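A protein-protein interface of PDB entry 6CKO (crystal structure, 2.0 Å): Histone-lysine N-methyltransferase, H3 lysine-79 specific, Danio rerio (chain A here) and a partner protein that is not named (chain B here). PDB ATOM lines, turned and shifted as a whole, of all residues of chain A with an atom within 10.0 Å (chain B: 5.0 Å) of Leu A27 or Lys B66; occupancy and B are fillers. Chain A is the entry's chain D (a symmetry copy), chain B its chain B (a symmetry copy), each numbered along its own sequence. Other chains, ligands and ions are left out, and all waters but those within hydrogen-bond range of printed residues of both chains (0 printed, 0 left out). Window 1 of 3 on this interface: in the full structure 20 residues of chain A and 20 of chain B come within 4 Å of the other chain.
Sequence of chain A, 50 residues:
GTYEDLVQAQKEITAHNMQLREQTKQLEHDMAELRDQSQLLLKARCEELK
Among the printed residues, pairs that only touch across the chains: Met A31 with Leu B69, Thr A24 with Ile B59, Met A31 with Lys B65, Leu A20 with Ile B59, Leu A27 with Lys B66, Leu A34 with Lys B66, Gln A23 with Ile B59, Arg A35 with Leu B69, Leu A27 with Thr B63, Ser A38 with Leu B69, Leu A34 with Gln B70 and Leu A27 with Ile B59.
Of the printed residues of chain B, Leu A27 touches Ile B59, Thr B63 and Lys B66. Lys B66 touches just these residues of chain A: Leu A27 (3.7 Å), Asp A30 (3.3 Å), Met A31 (3.5 Å) and Leu A34 (3.7 Å). Printed residues of chain A within 4 Å of Thr B63: Leu A27. Ala B64 touches none of the printed residues of chain A. Of the printed residues of chain B, Ser A38 touches Leu B69 (3.9 Å). Printed residues of chain B within 4 Å of Gln A23: Ile B59 (3.7 Å). Of the printed residues of chain B, Leu A34 touches Lys B66 and Gln B70. The nearest residue of chain A that does not touch Lys B66 is Gln A26 (6.4 Å).
N of Lys B66 sits at hydrogen-bond distance from SD of Met A31, 3.5 Å away. OD2 of Asp A30 is in salt-bridge range of NZ of Lys B66.
The backbone carbonyl oxygen (O) of Ile B59 lies within hydrogen-bond range of the side-chain hydroxyl (OG1) of Thr B63. O of Leu A20 is in hydrogen-bond range of OG1 of Thr A24 (2.8 Å). The backbone carbonyl oxygen (O) of Leu A34 is in hydrogen-bond range of the side-chain hydroxyl (OG) of Ser A38, 3.3 Å away. OD1 of Asp A30 sits at hydrogen-bond distance from NE2 of Gln A26.
Hydrophobic or aromatic side chains of chain B that line the printed part of chain A: Ile B59 and Leu B69. Of the 18 printed residues of chain A, 9 touch a printed residue of chain B. Printed residues of chain A that touch a printed residue of chain B: Leu A20, Gln A23, Thr A24, Leu A27, Asp A30, Met A31, Leu A34, Arg A35 and Ser A38. Hydrophobic or aromatic side chains of chain A within 4 Å of the printed part of chain B: Leu A20, Leu A27, Met A31 and Leu A34. Among the printed residues, 14 pairs touch across the chains.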
ATOM      1  N   GLN A  19       0.836  -6.480  11.373  1.00  0.00           N
ATOM      2  CA  GLN A  19       1.400  -7.256  10.304  1.00  0.00           C
ATOM      3  C   GLN A  19       0.305  -7.810   9.336  1.00  0.00           C
ATOM      4  O   GLN A  19       0.459  -7.770   8.084  1.00  0.00           O
ATOM      5  CB  GLN A  19       2.280  -8.392  10.881  1.00  0.00           C
ATOM      6  N   LEU A  20      -0.782  -8.318   9.908  1.00  0.00           N
ATOM      7  CA  LEU A  20      -1.883  -8.820   9.116  1.00  0.00           C
ATOM      8  C   LEU A  20      -2.559  -7.710   8.289  1.00  0.00           C
ATOM      9  O   LEU A  20      -2.927  -7.946   7.131  1.00  0.00           O
ATOM     10  CB  LEU A  20      -2.898  -9.554   9.962  1.00  0.00           C
ATOM     11  CG  LEU A  20      -2.357 -10.827  10.611  1.00  0.00           C
ATOM     12  CD1 LEU A  20      -3.388 -11.318  11.621  1.00  0.00           C
ATOM     13  CD2 LEU A  20      -2.014 -11.895   9.585  1.00  0.00           C
ATOM     14  N   ARG A  21      -2.696  -6.530   8.874  1.00  0.00           N
ATOM     15  CA  ARG A  21      -3.204  -5.389   8.157  1.00  0.00           C
ATOM     16  C   ARG A  21      -2.279  -5.009   6.969  1.00  0.00           C
ATOM     17  O   ARG A  21      -2.788  -4.800   5.867  1.00  0.00           O
ATOM     18  CB  ARG A  21      -3.401  -4.199   9.066  1.00  0.00           C
ATOM     19  CG  ARG A  21      -4.688  -4.275   9.860  1.00  0.00           C
ATOM     20  CD  ARG A  21      -4.642  -3.256  10.954  1.00  0.00           C
ATOM     21  NE  ARG A  21      -5.771  -3.295  11.861  1.00  0.00           N
ATOM     22  CZ  ARG A  21      -6.951  -2.688  11.669  1.00  0.00           C
ATOM     23  NH1 ARG A  21      -7.221  -2.031  10.537  1.00  0.00           N
ATOM     24  NH2 ARG A  21      -7.890  -2.747  12.632  1.00  0.00           N
ATOM     25  N   GLU A  22      -0.961  -4.942   7.202  1.00  0.00           N
ATOM     26  CA  GLU A  22      -0.036  -4.589   6.122  1.00  0.00           C
ATOM     27  C   GLU A  22      -0.141  -5.603   4.987  1.00  0.00           C
ATOM     28  O   GLU A  22      -0.192  -5.251   3.822  1.00  0.00           O
ATOM     29  CB  GLU A  22       1.404  -4.518   6.624  1.00  0.00           C
ATOM     30  N   GLN A  23      -0.187  -6.877   5.355  1.00  0.00           N
ATOM     31  CA  GLN A  23      -0.236  -7.930   4.375  1.00  0.00           C
ATOM     32  C   GLN A  23      -1.534  -7.868   3.541  1.00  0.00           C
ATOM     33  O   GLN A  23      -1.510  -7.982   2.301  1.00  0.00           O
ATOM     34  CB  GLN A  23      -0.052  -9.263   5.081  1.00  0.00           C
ATOM     35  CG  GLN A  23       0.278 -10.390   4.170  1.00  0.00           C
ATOM     36  CD  GLN A  23       0.502 -11.698   4.899  1.00  0.00           C
ATOM     37  OE1 GLN A  23       0.713 -11.734   6.115  1.00  0.00           O
ATOM     38  NE2 GLN A  23       0.500 -12.774   4.138  1.00  0.00           N
ATOM     39  N   THR A  24      -2.635  -7.600   4.226  1.00  0.00           N
ATOM     40  CA  THR A  24      -3.941  -7.432   3.625  1.00  0.00           C
ATOM     41  C   THR A  24      -4.013  -6.201   2.700  1.00  0.00           C
ATOM     42  O   THR A  24      -4.579  -6.288   1.618  1.00  0.00           O
ATOM     43  CB  THR A  24      -5.037  -7.348   4.725  1.00  0.00           C
ATOM     44  OG1 THR A  24      -5.054  -8.584   5.440  1.00  0.00           O
ATOM     45  CG2 THR A  24      -6.415  -7.142   4.128  1.00  0.00           C
ATOM     46  N   LYS A  25      -3.407  -5.088   3.101  1.00  0.00           N
ATOM     47  CA  LYS A  25      -3.333  -3.911   2.245  1.00  0.00           C
ATOM     48  C   LYS A  25      -2.578  -4.226   0.928  1.00  0.00           C
ATOM     49  O   LYS A  25      -3.060  -3.867  -0.162  1.00  0.00           O
ATOM     50  CB  LYS A  25      -2.667  -2.768   3.016  1.00  0.00           C
ATOM     51  CG  LYS A  25      -2.467  -1.510   2.201  1.00  0.00           C
ATOM     52  N   GLN A  26      -1.439  -4.919   1.037  1.00  0.00           N
ATOM     53  CA  GLN A  26      -0.630  -5.254  -0.131  1.00  0.00           C
ATOM     54  C   GLN A  26      -1.367  -6.242  -1.066  1.00  0.00           C
ATOM     55  O   GLN A  26      -1.366  -6.067  -2.303  1.00  0.00           O
ATOM     56  CB  GLN A  26       0.762  -5.767   0.273  1.00  0.00           C
ATOM     57  CG  GLN A  26       1.670  -6.183  -0.892  1.00  0.00           C
ATOM     58  CD  GLN A  26       2.005  -5.038  -1.831  1.00  0.00           C
ATOM     59  OE1 GLN A  26       2.258  -3.936  -1.359  1.00  0.00           O
ATOM     60  NE2 GLN A  26       2.127  -5.312  -3.158  1.00  0.00           N
ATOM     61  N   LEU A  27      -1.985  -7.248  -0.482  1.00  0.00           N
ATOM     62  CA  LEU A  27      -2.784  -8.195  -1.223  1.00  0.00           C
ATOM     63  C   LEU A  27      -3.957  -7.567  -1.979  1.00  0.00           C
ATOM     64  O   LEU A  27      -4.158  -7.902  -3.138  1.00  0.00           O
ATOM     65  CB  LEU A  27      -3.272  -9.325  -0.334  1.00  0.00           C
ATOM     66  CG  LEU A  27      -2.332 -10.480  -0.139  1.00  0.00           C
ATOM     67  CD1 LEU A  27      -2.896 -11.344   0.980  1.00  0.00           C
ATOM     68  CD2 LEU A  27      -2.215 -11.314  -1.405  1.00  0.00           C
ATOM     69  N   GLU A  28      -4.700  -6.669  -1.330  1.00  0.00           N
ATOM     70  CA  GLU A  28      -5.707  -5.843  -1.995  1.00  0.00           C
ATOM     71  C   GLU A  28      -5.163  -4.983  -3.131  1.00  0.00           C
ATOM     72  O   GLU A  28      -5.813  -4.868  -4.169  1.00  0.00           O
ATOM     73  CB  GLU A  28      -6.445  -4.969  -1.006  1.00  0.00           C
ATOM     74  CG  GLU A  28      -7.447  -5.818  -0.229  1.00  0.00           C
ATOM     75  CD  GLU A  28      -8.052  -5.130   0.986  1.00  0.00           C
ATOM     76  OE1 GLU A  28      -7.852  -3.904   1.198  1.00  0.00           O
ATOM     77  OE2 GLU A  28      -8.734  -5.847   1.759  1.00  0.00           O
ATOM     78  N   HIS A  29      -3.984  -4.399  -2.921  1.00  0.00           N
ATOM     79  CA  HIS A  29      -3.344  -3.662  -3.969  1.00  0.00           C
ATOM     80  C   HIS A  29      -2.941  -4.607  -5.145  1.00  0.00           C
ATOM     81  O   HIS A  29      -3.196  -4.259  -6.269  1.00  0.00           O
ATOM     82  CB  HIS A  29      -2.157  -2.845  -3.463  1.00  0.00           C
ATOM     83  CG  HIS A  29      -1.376  -2.173  -4.555  1.00  0.00           C
ATOM     84  ND1 HIS A  29      -1.854  -1.094  -5.259  1.00  0.00           N
ATOM     85  CD2 HIS A  29      -0.118  -2.381  -4.998  1.00  0.00           C
ATOM     86  CE1 HIS A  29      -0.933  -0.676  -6.103  1.00  0.00           C
ATOM     87  NE2 HIS A  29       0.126  -1.452  -5.975  1.00  0.00           N
ATOM     88  N   ASP A  30      -2.334  -5.761  -4.853  1.00  0.00           N
ATOM     89  CA  ASP A  30      -1.972  -6.743  -5.848  1.00  0.00           C
ATOM     90  C   ASP A  30      -3.216  -7.098  -6.658  1.00  0.00           C
ATOM     91  O   ASP A  30      -3.154  -7.173  -7.903  1.00  0.00           O
ATOM     92  CB  ASP A  30      -1.445  -8.084  -5.269  1.00  0.00           C
ATOM     93  CG  ASP A  30      -0.101  -7.989  -4.526  1.00  0.00           C
ATOM     94  OD1 ASP A  30       0.716  -7.141  -4.837  1.00  0.00           O
ATOM     95  OD2 ASP A  30       0.108  -8.832  -3.575  1.00  0.00           O
ATOM     96  N   MET A  31      -4.331  -7.351  -5.973  1.00  0.00           N
ATOM     97  CA  MET A  31      -5.565  -7.772  -6.625  1.00  0.00           C
ATOM     98  C   MET A  31      -6.097  -6.695  -7.516  1.00  0.00           C
ATOM     99  O   MET A  31      -6.557  -7.010  -8.612  1.00  0.00           O
ATOM    100  CB  MET A  31      -6.683  -8.136  -5.644  1.00  0.00           C
ATOM    101  CG  MET A  31      -6.492  -9.467  -4.918  1.00  0.00           C
ATOM    102  SD  MET A  31      -6.572 -10.874  -6.032  1.00  0.00           S
ATOM    103  CE  MET A  31      -8.307 -10.842  -6.482  1.00  0.00           C
ATOM    104  N   ALA A  32      -6.069  -5.440  -7.049  1.00  0.00           N
ATOM    105  CA  ALA A  32      -6.528  -4.309  -7.862  1.00  0.00           C
ATOM    106  C   ALA A  32      -5.713  -4.209  -9.157  1.00  0.00           C
ATOM    107  O   ALA A  32      -6.309  -4.119 -10.236  1.00  0.00           O
ATOM    108  CB  ALA A  32      -6.503  -2.977  -7.089  1.00  0.00           C
ATOM    109  N   GLU A  33      -4.381  -4.323  -9.059  1.00  0.00           N
ATOM    110  CA  GLU A  33      -3.525  -4.254 -10.238  1.00  0.00           C
ATOM    111  C   GLU A  33      -3.814  -5.394 -11.210  1.00  0.00           C
ATOM    112  O   GLU A  33      -3.878  -5.182 -12.410  1.00  0.00           O
ATOM    113  CB  GLU A  33      -2.043  -4.278  -9.867  1.00  0.00           C
ATOM    114  CG  GLU A  33      -1.571  -3.067  -9.063  1.00  0.00           C
ATOM    115  CD  GLU A  33      -1.663  -1.777  -9.833  1.00  0.00           C
ATOM    116  OE1 GLU A  33      -1.430  -1.817 -11.029  1.00  0.00           O
ATOM    117  OE2 GLU A  33      -1.944  -0.722  -9.236  1.00  0.00           O
ATOM    118  N   LEU A  34      -3.942  -6.606 -10.678  1.00  0.00           N
ATOM    119  CA  LEU A  34      -4.281  -7.776 -11.499  1.00  0.00           C
ATOM    120  C   LEU A  34      -5.672  -7.715 -12.164  1.00  0.00           C
ATOM    121  O   LEU A  34      -5.803  -8.077 -13.337  1.00  0.00           O
ATOM    122  CB  LEU A  34      -4.101  -9.080 -10.725  1.00  0.00           C
ATOM    123  CG  LEU A  34      -2.683  -9.409 -10.330  1.00  0.00           C
ATOM    124  CD1 LEU A  34      -2.639 -10.504  -9.284  1.00  0.00           C
ATOM    125  CD2 LEU A  34      -1.861  -9.824 -11.525  1.00  0.00           C
ATOM    126  N   ARG A  35      -6.676  -7.241 -11.457  1.00  0.00           N
ATOM    127  CA  ARG A  35      -7.996  -7.018 -12.049  1.00  0.00           C
ATOM    128  C   ARG A  35      -7.970  -5.948 -13.156  1.00  0.00           C
ATOM    129  O   ARG A  35      -8.753  -6.042 -14.091  1.00  0.00           O
ATOM    130  CB  ARG A  35      -9.046  -6.597 -11.032  1.00  0.00           C
ATOM    131  CG  ARG A  35      -9.516  -7.723 -10.143  1.00  0.00           C
ATOM    132  CD  ARG A  35     -10.771  -7.294  -9.400  1.00  0.00           C
ATOM    133  NE  ARG A  35     -10.475  -6.155  -8.535  1.00  0.00           N
ATOM    134  CZ  ARG A  35     -10.125  -6.212  -7.243  1.00  0.00           C
ATOM    135  NH1 ARG A  35     -10.023  -7.370  -6.588  1.00  0.00           N
ATOM    136  NH2 ARG A  35      -9.884  -5.082  -6.594  1.00  0.00           N
ATOM    137  N   SER A  38      -6.852  -7.762 -16.053  1.00  0.00           N
ATOM    138  CA  SER A  38      -7.949  -8.664 -16.501  1.00  0.00           C
ATOM    139  C   SER A  38      -8.947  -7.919 -17.382  1.00  0.00           C
ATOM    140  O   SER A  38      -9.250  -8.377 -18.441  1.00  0.00           O
ATOM    141  CB  SER A  38      -8.740  -9.301 -15.351  1.00  0.00           C
ATOM    142  OG  SER A  38      -7.948 -10.244 -14.656  1.00  0.00           O
ATOM    143  N   ILE B  59      -6.688 -13.168   4.021  1.00  0.00           N
ATOM    144  CA  ILE B  59      -5.366 -13.435   3.424  1.00  0.00           C
ATOM    145  C   ILE B  59      -5.368 -14.740   2.617  1.00  0.00           C
ATOM    146  O   ILE B  59      -4.921 -14.756   1.448  1.00  0.00           O
ATOM    147  CB  ILE B  59      -4.237 -13.408   4.490  1.00  0.00           C
ATOM    148  CG1 ILE B  59      -3.918 -11.954   4.844  1.00  0.00           C
ATOM    149  CG2 ILE B  59      -2.985 -14.134   4.051  1.00  0.00           C
ATOM    150  CD1 ILE B  59      -3.116 -11.762   6.115  1.00  0.00           C
ATOM    151  N   LEU B  62      -7.611 -14.123  -0.521  1.00  0.00           N
ATOM    152  CA  LEU B  62      -6.964 -13.215  -1.448  1.00  0.00           C
ATOM    153  C   LEU B  62      -5.741 -13.847  -2.083  1.00  0.00           C
ATOM    154  O   LEU B  62      -5.530 -13.678  -3.280  1.00  0.00           O
ATOM    155  CB  LEU B  62      -6.612 -11.887  -0.789  1.00  0.00           C
ATOM    156  CG  LEU B  62      -7.767 -10.985  -0.372  1.00  0.00           C
ATOM    157  CD1 LEU B  62      -7.241  -9.854   0.481  1.00  0.00           C
ATOM    158  CD2 LEU B  62      -8.517 -10.375  -1.525  1.00  0.00           C
ATOM    159  N   THR B  63      -4.987 -14.646  -1.338  1.00  0.00           N
ATOM    160  CA  THR B  63      -3.839 -15.359  -1.902  1.00  0.00           C
ATOM    161  C   THR B  63      -4.232 -16.347  -3.019  1.00  0.00           C
ATOM    162  O   THR B  63      -3.594 -16.348  -4.102  1.00  0.00           O
ATOM    163  CB  THR B  63      -2.967 -16.067  -0.830  1.00  0.00           C
ATOM    164  OG1 THR B  63      -2.537 -15.101   0.136  1.00  0.00           O
ATOM    165  CG2 THR B  63      -1.747 -16.712  -1.459  1.00  0.00           C
ATOM    166  N   ALA B  64      -5.248 -17.190  -2.765  1.00  0.00           N
ATOM    167  CA  ALA B  64      -5.788 -18.044  -3.829  1.00  0.00           C
ATOM    168  C   ALA B  64      -6.342 -17.255  -5.039  1.00  0.00           C
ATOM    169  O   ALA B  64      -6.103 -17.658  -6.170  1.00  0.00           O
ATOM    170  CB  ALA B  64      -6.869 -18.972  -3.283  1.00  0.00           C
ATOM    171  N   LYS B  65      -7.093 -16.179  -4.798  1.00  0.00           N
ATOM    172  CA  LYS B  65      -7.663 -15.367  -5.876  1.00  0.00           C
ATOM    173  C   LYS B  65      -6.582 -14.722  -6.763  1.00  0.00           C
ATOM    174  O   LYS B  65      -6.701 -14.708  -7.987  1.00  0.00           O
ATOM    175  CB  LYS B  65      -8.599 -14.269  -5.341  1.00  0.00           C
ATOM    176  CG  LYS B  65     -10.059 -14.672  -5.137  1.00  0.00           C
ATOM    177  CD  LYS B  65     -10.945 -13.522  -4.589  1.00  0.00           C
ATOM    178  CE  LYS B  65     -12.280 -14.023  -4.017  1.00  0.00           C
ATOM    179  N   LYS B  66      -5.539 -14.185  -6.123  1.00  0.00           N
ATOM    180  CA  LYS B  66      -4.412 -13.618  -6.808  1.00  0.00           C
ATOM    181  C   LYS B  66      -3.786 -14.615  -7.788  1.00  0.00           C
ATOM    182  O   LYS B  66      -3.528 -14.265  -8.965  1.00  0.00           O
ATOM    183  CB  LYS B  66      -3.423 -13.077  -5.778  1.00  0.00           C
ATOM    184  CG  LYS B  66      -2.092 -12.664  -6.314  1.00  0.00           C
ATOM    185  CD  LYS B  66      -1.280 -11.938  -5.260  1.00  0.00           C
ATOM    186  CE  LYS B  66      -0.571 -12.880  -4.330  1.00  0.00           C
ATOM    187  NZ  LYS B  66       0.505 -12.066  -3.732  1.00  0.00           N
ATOM    188  N   GLU B  67      -3.564 -15.855  -7.328  1.00  0.00           N
ATOM    189  CA  GLU B  67      -2.987 -16.891  -8.188  1.00  0.00           C
ATOM    190  C   GLU B  67      -3.919 -17.228  -9.375  1.00  0.00           C
ATOM    191  O   GLU B  67      -3.430 -17.405 -10.501  1.00  0.00           O
ATOM    192  CB  GLU B  67      -2.673 -18.188  -7.406  1.00  0.00           C
ATOM    193  N   ARG B  68      -5.242 -17.257  -9.143  1.00  0.00           N
ATOM    194  CA  ARG B  68      -6.203 -17.498 -10.251  1.00  0.00           C
ATOM    195  C   ARG B  68      -6.236 -16.355 -11.247  1.00  0.00           C
ATOM    196  O   ARG B  68      -6.361 -16.587 -12.452  1.00  0.00           O
ATOM    197  CB  ARG B  68      -7.613 -17.802  -9.710  1.00  0.00           C
ATOM    198  CG  ARG B  68      -7.638 -19.134  -8.969  1.00  0.00           C
ATOM    199  CD  ARG B  68      -9.045 -19.586  -8.644  1.00  0.00           C
ATOM    200  NE  ARG B  68      -9.775 -18.624  -7.851  1.00  0.00           N
ATOM    201  CZ  ARG B  68      -9.904 -18.658  -6.519  1.00  0.00           C
ATOM    202  NH1 ARG B  68     -10.625 -17.721  -5.933  1.00  0.00           N
ATOM    203  NH2 ARG B  68      -9.332 -19.605  -5.762  1.00  0.00           N
ATOM    204  N   LEU B  69      -6.074 -15.130 -10.769  1.00  0.00           N
ATOM    205  CA  LEU B  69      -5.983 -13.983 -11.684  1.00  0.00           C
ATOM    206  C   LEU B  69      -4.706 -14.001 -12.510  1.00  0.00           C
ATOM    207  O   LEU B  69      -4.758 -13.741 -13.713  1.00  0.00           O
ATOM    208  CB  LEU B  69      -6.171 -12.658 -10.972  1.00  0.00           C
ATOM    209  CG  LEU B  69      -7.578 -12.372 -10.451  1.00  0.00           C
ATOM    210  CD1 LEU B  69      -7.590 -10.998  -9.815  1.00  0.00           C
ATOM    211  CD2 LEU B  69      -8.620 -12.456 -11.536  1.00  0.00           C
ATOM    212  N   GLN B  70      -3.588 -14.402 -11.906  1.00  0.00           N
ATOM    213  CA  GLN B  70      -2.324 -14.565 -12.642  1.00  0.00           C
ATOM    214  C   GLN B  70      -2.533 -15.522 -13.827  1.00  0.00           C
ATOM    215  O   GLN B  70      -2.133 -15.195 -14.926  1.00  0.00           O
ATOM    216  CB  GLN B  70      -1.169 -15.028 -11.758  1.00  0.00           C
ATOM    217  CG  GLN B  70      -0.676 -13.979 -10.759  1.00  0.00           C
ATOM    218  CD  GLN B  70       0.371 -13.016 -11.332  1.00  0.00           C
ATOM    219  OE1 GLN B  70       0.483 -12.879 -12.550  1.00  0.00           O
ATOM    220  NE2 GLN B  70       1.175 -12.371 -10.445  1.00  0.00           N
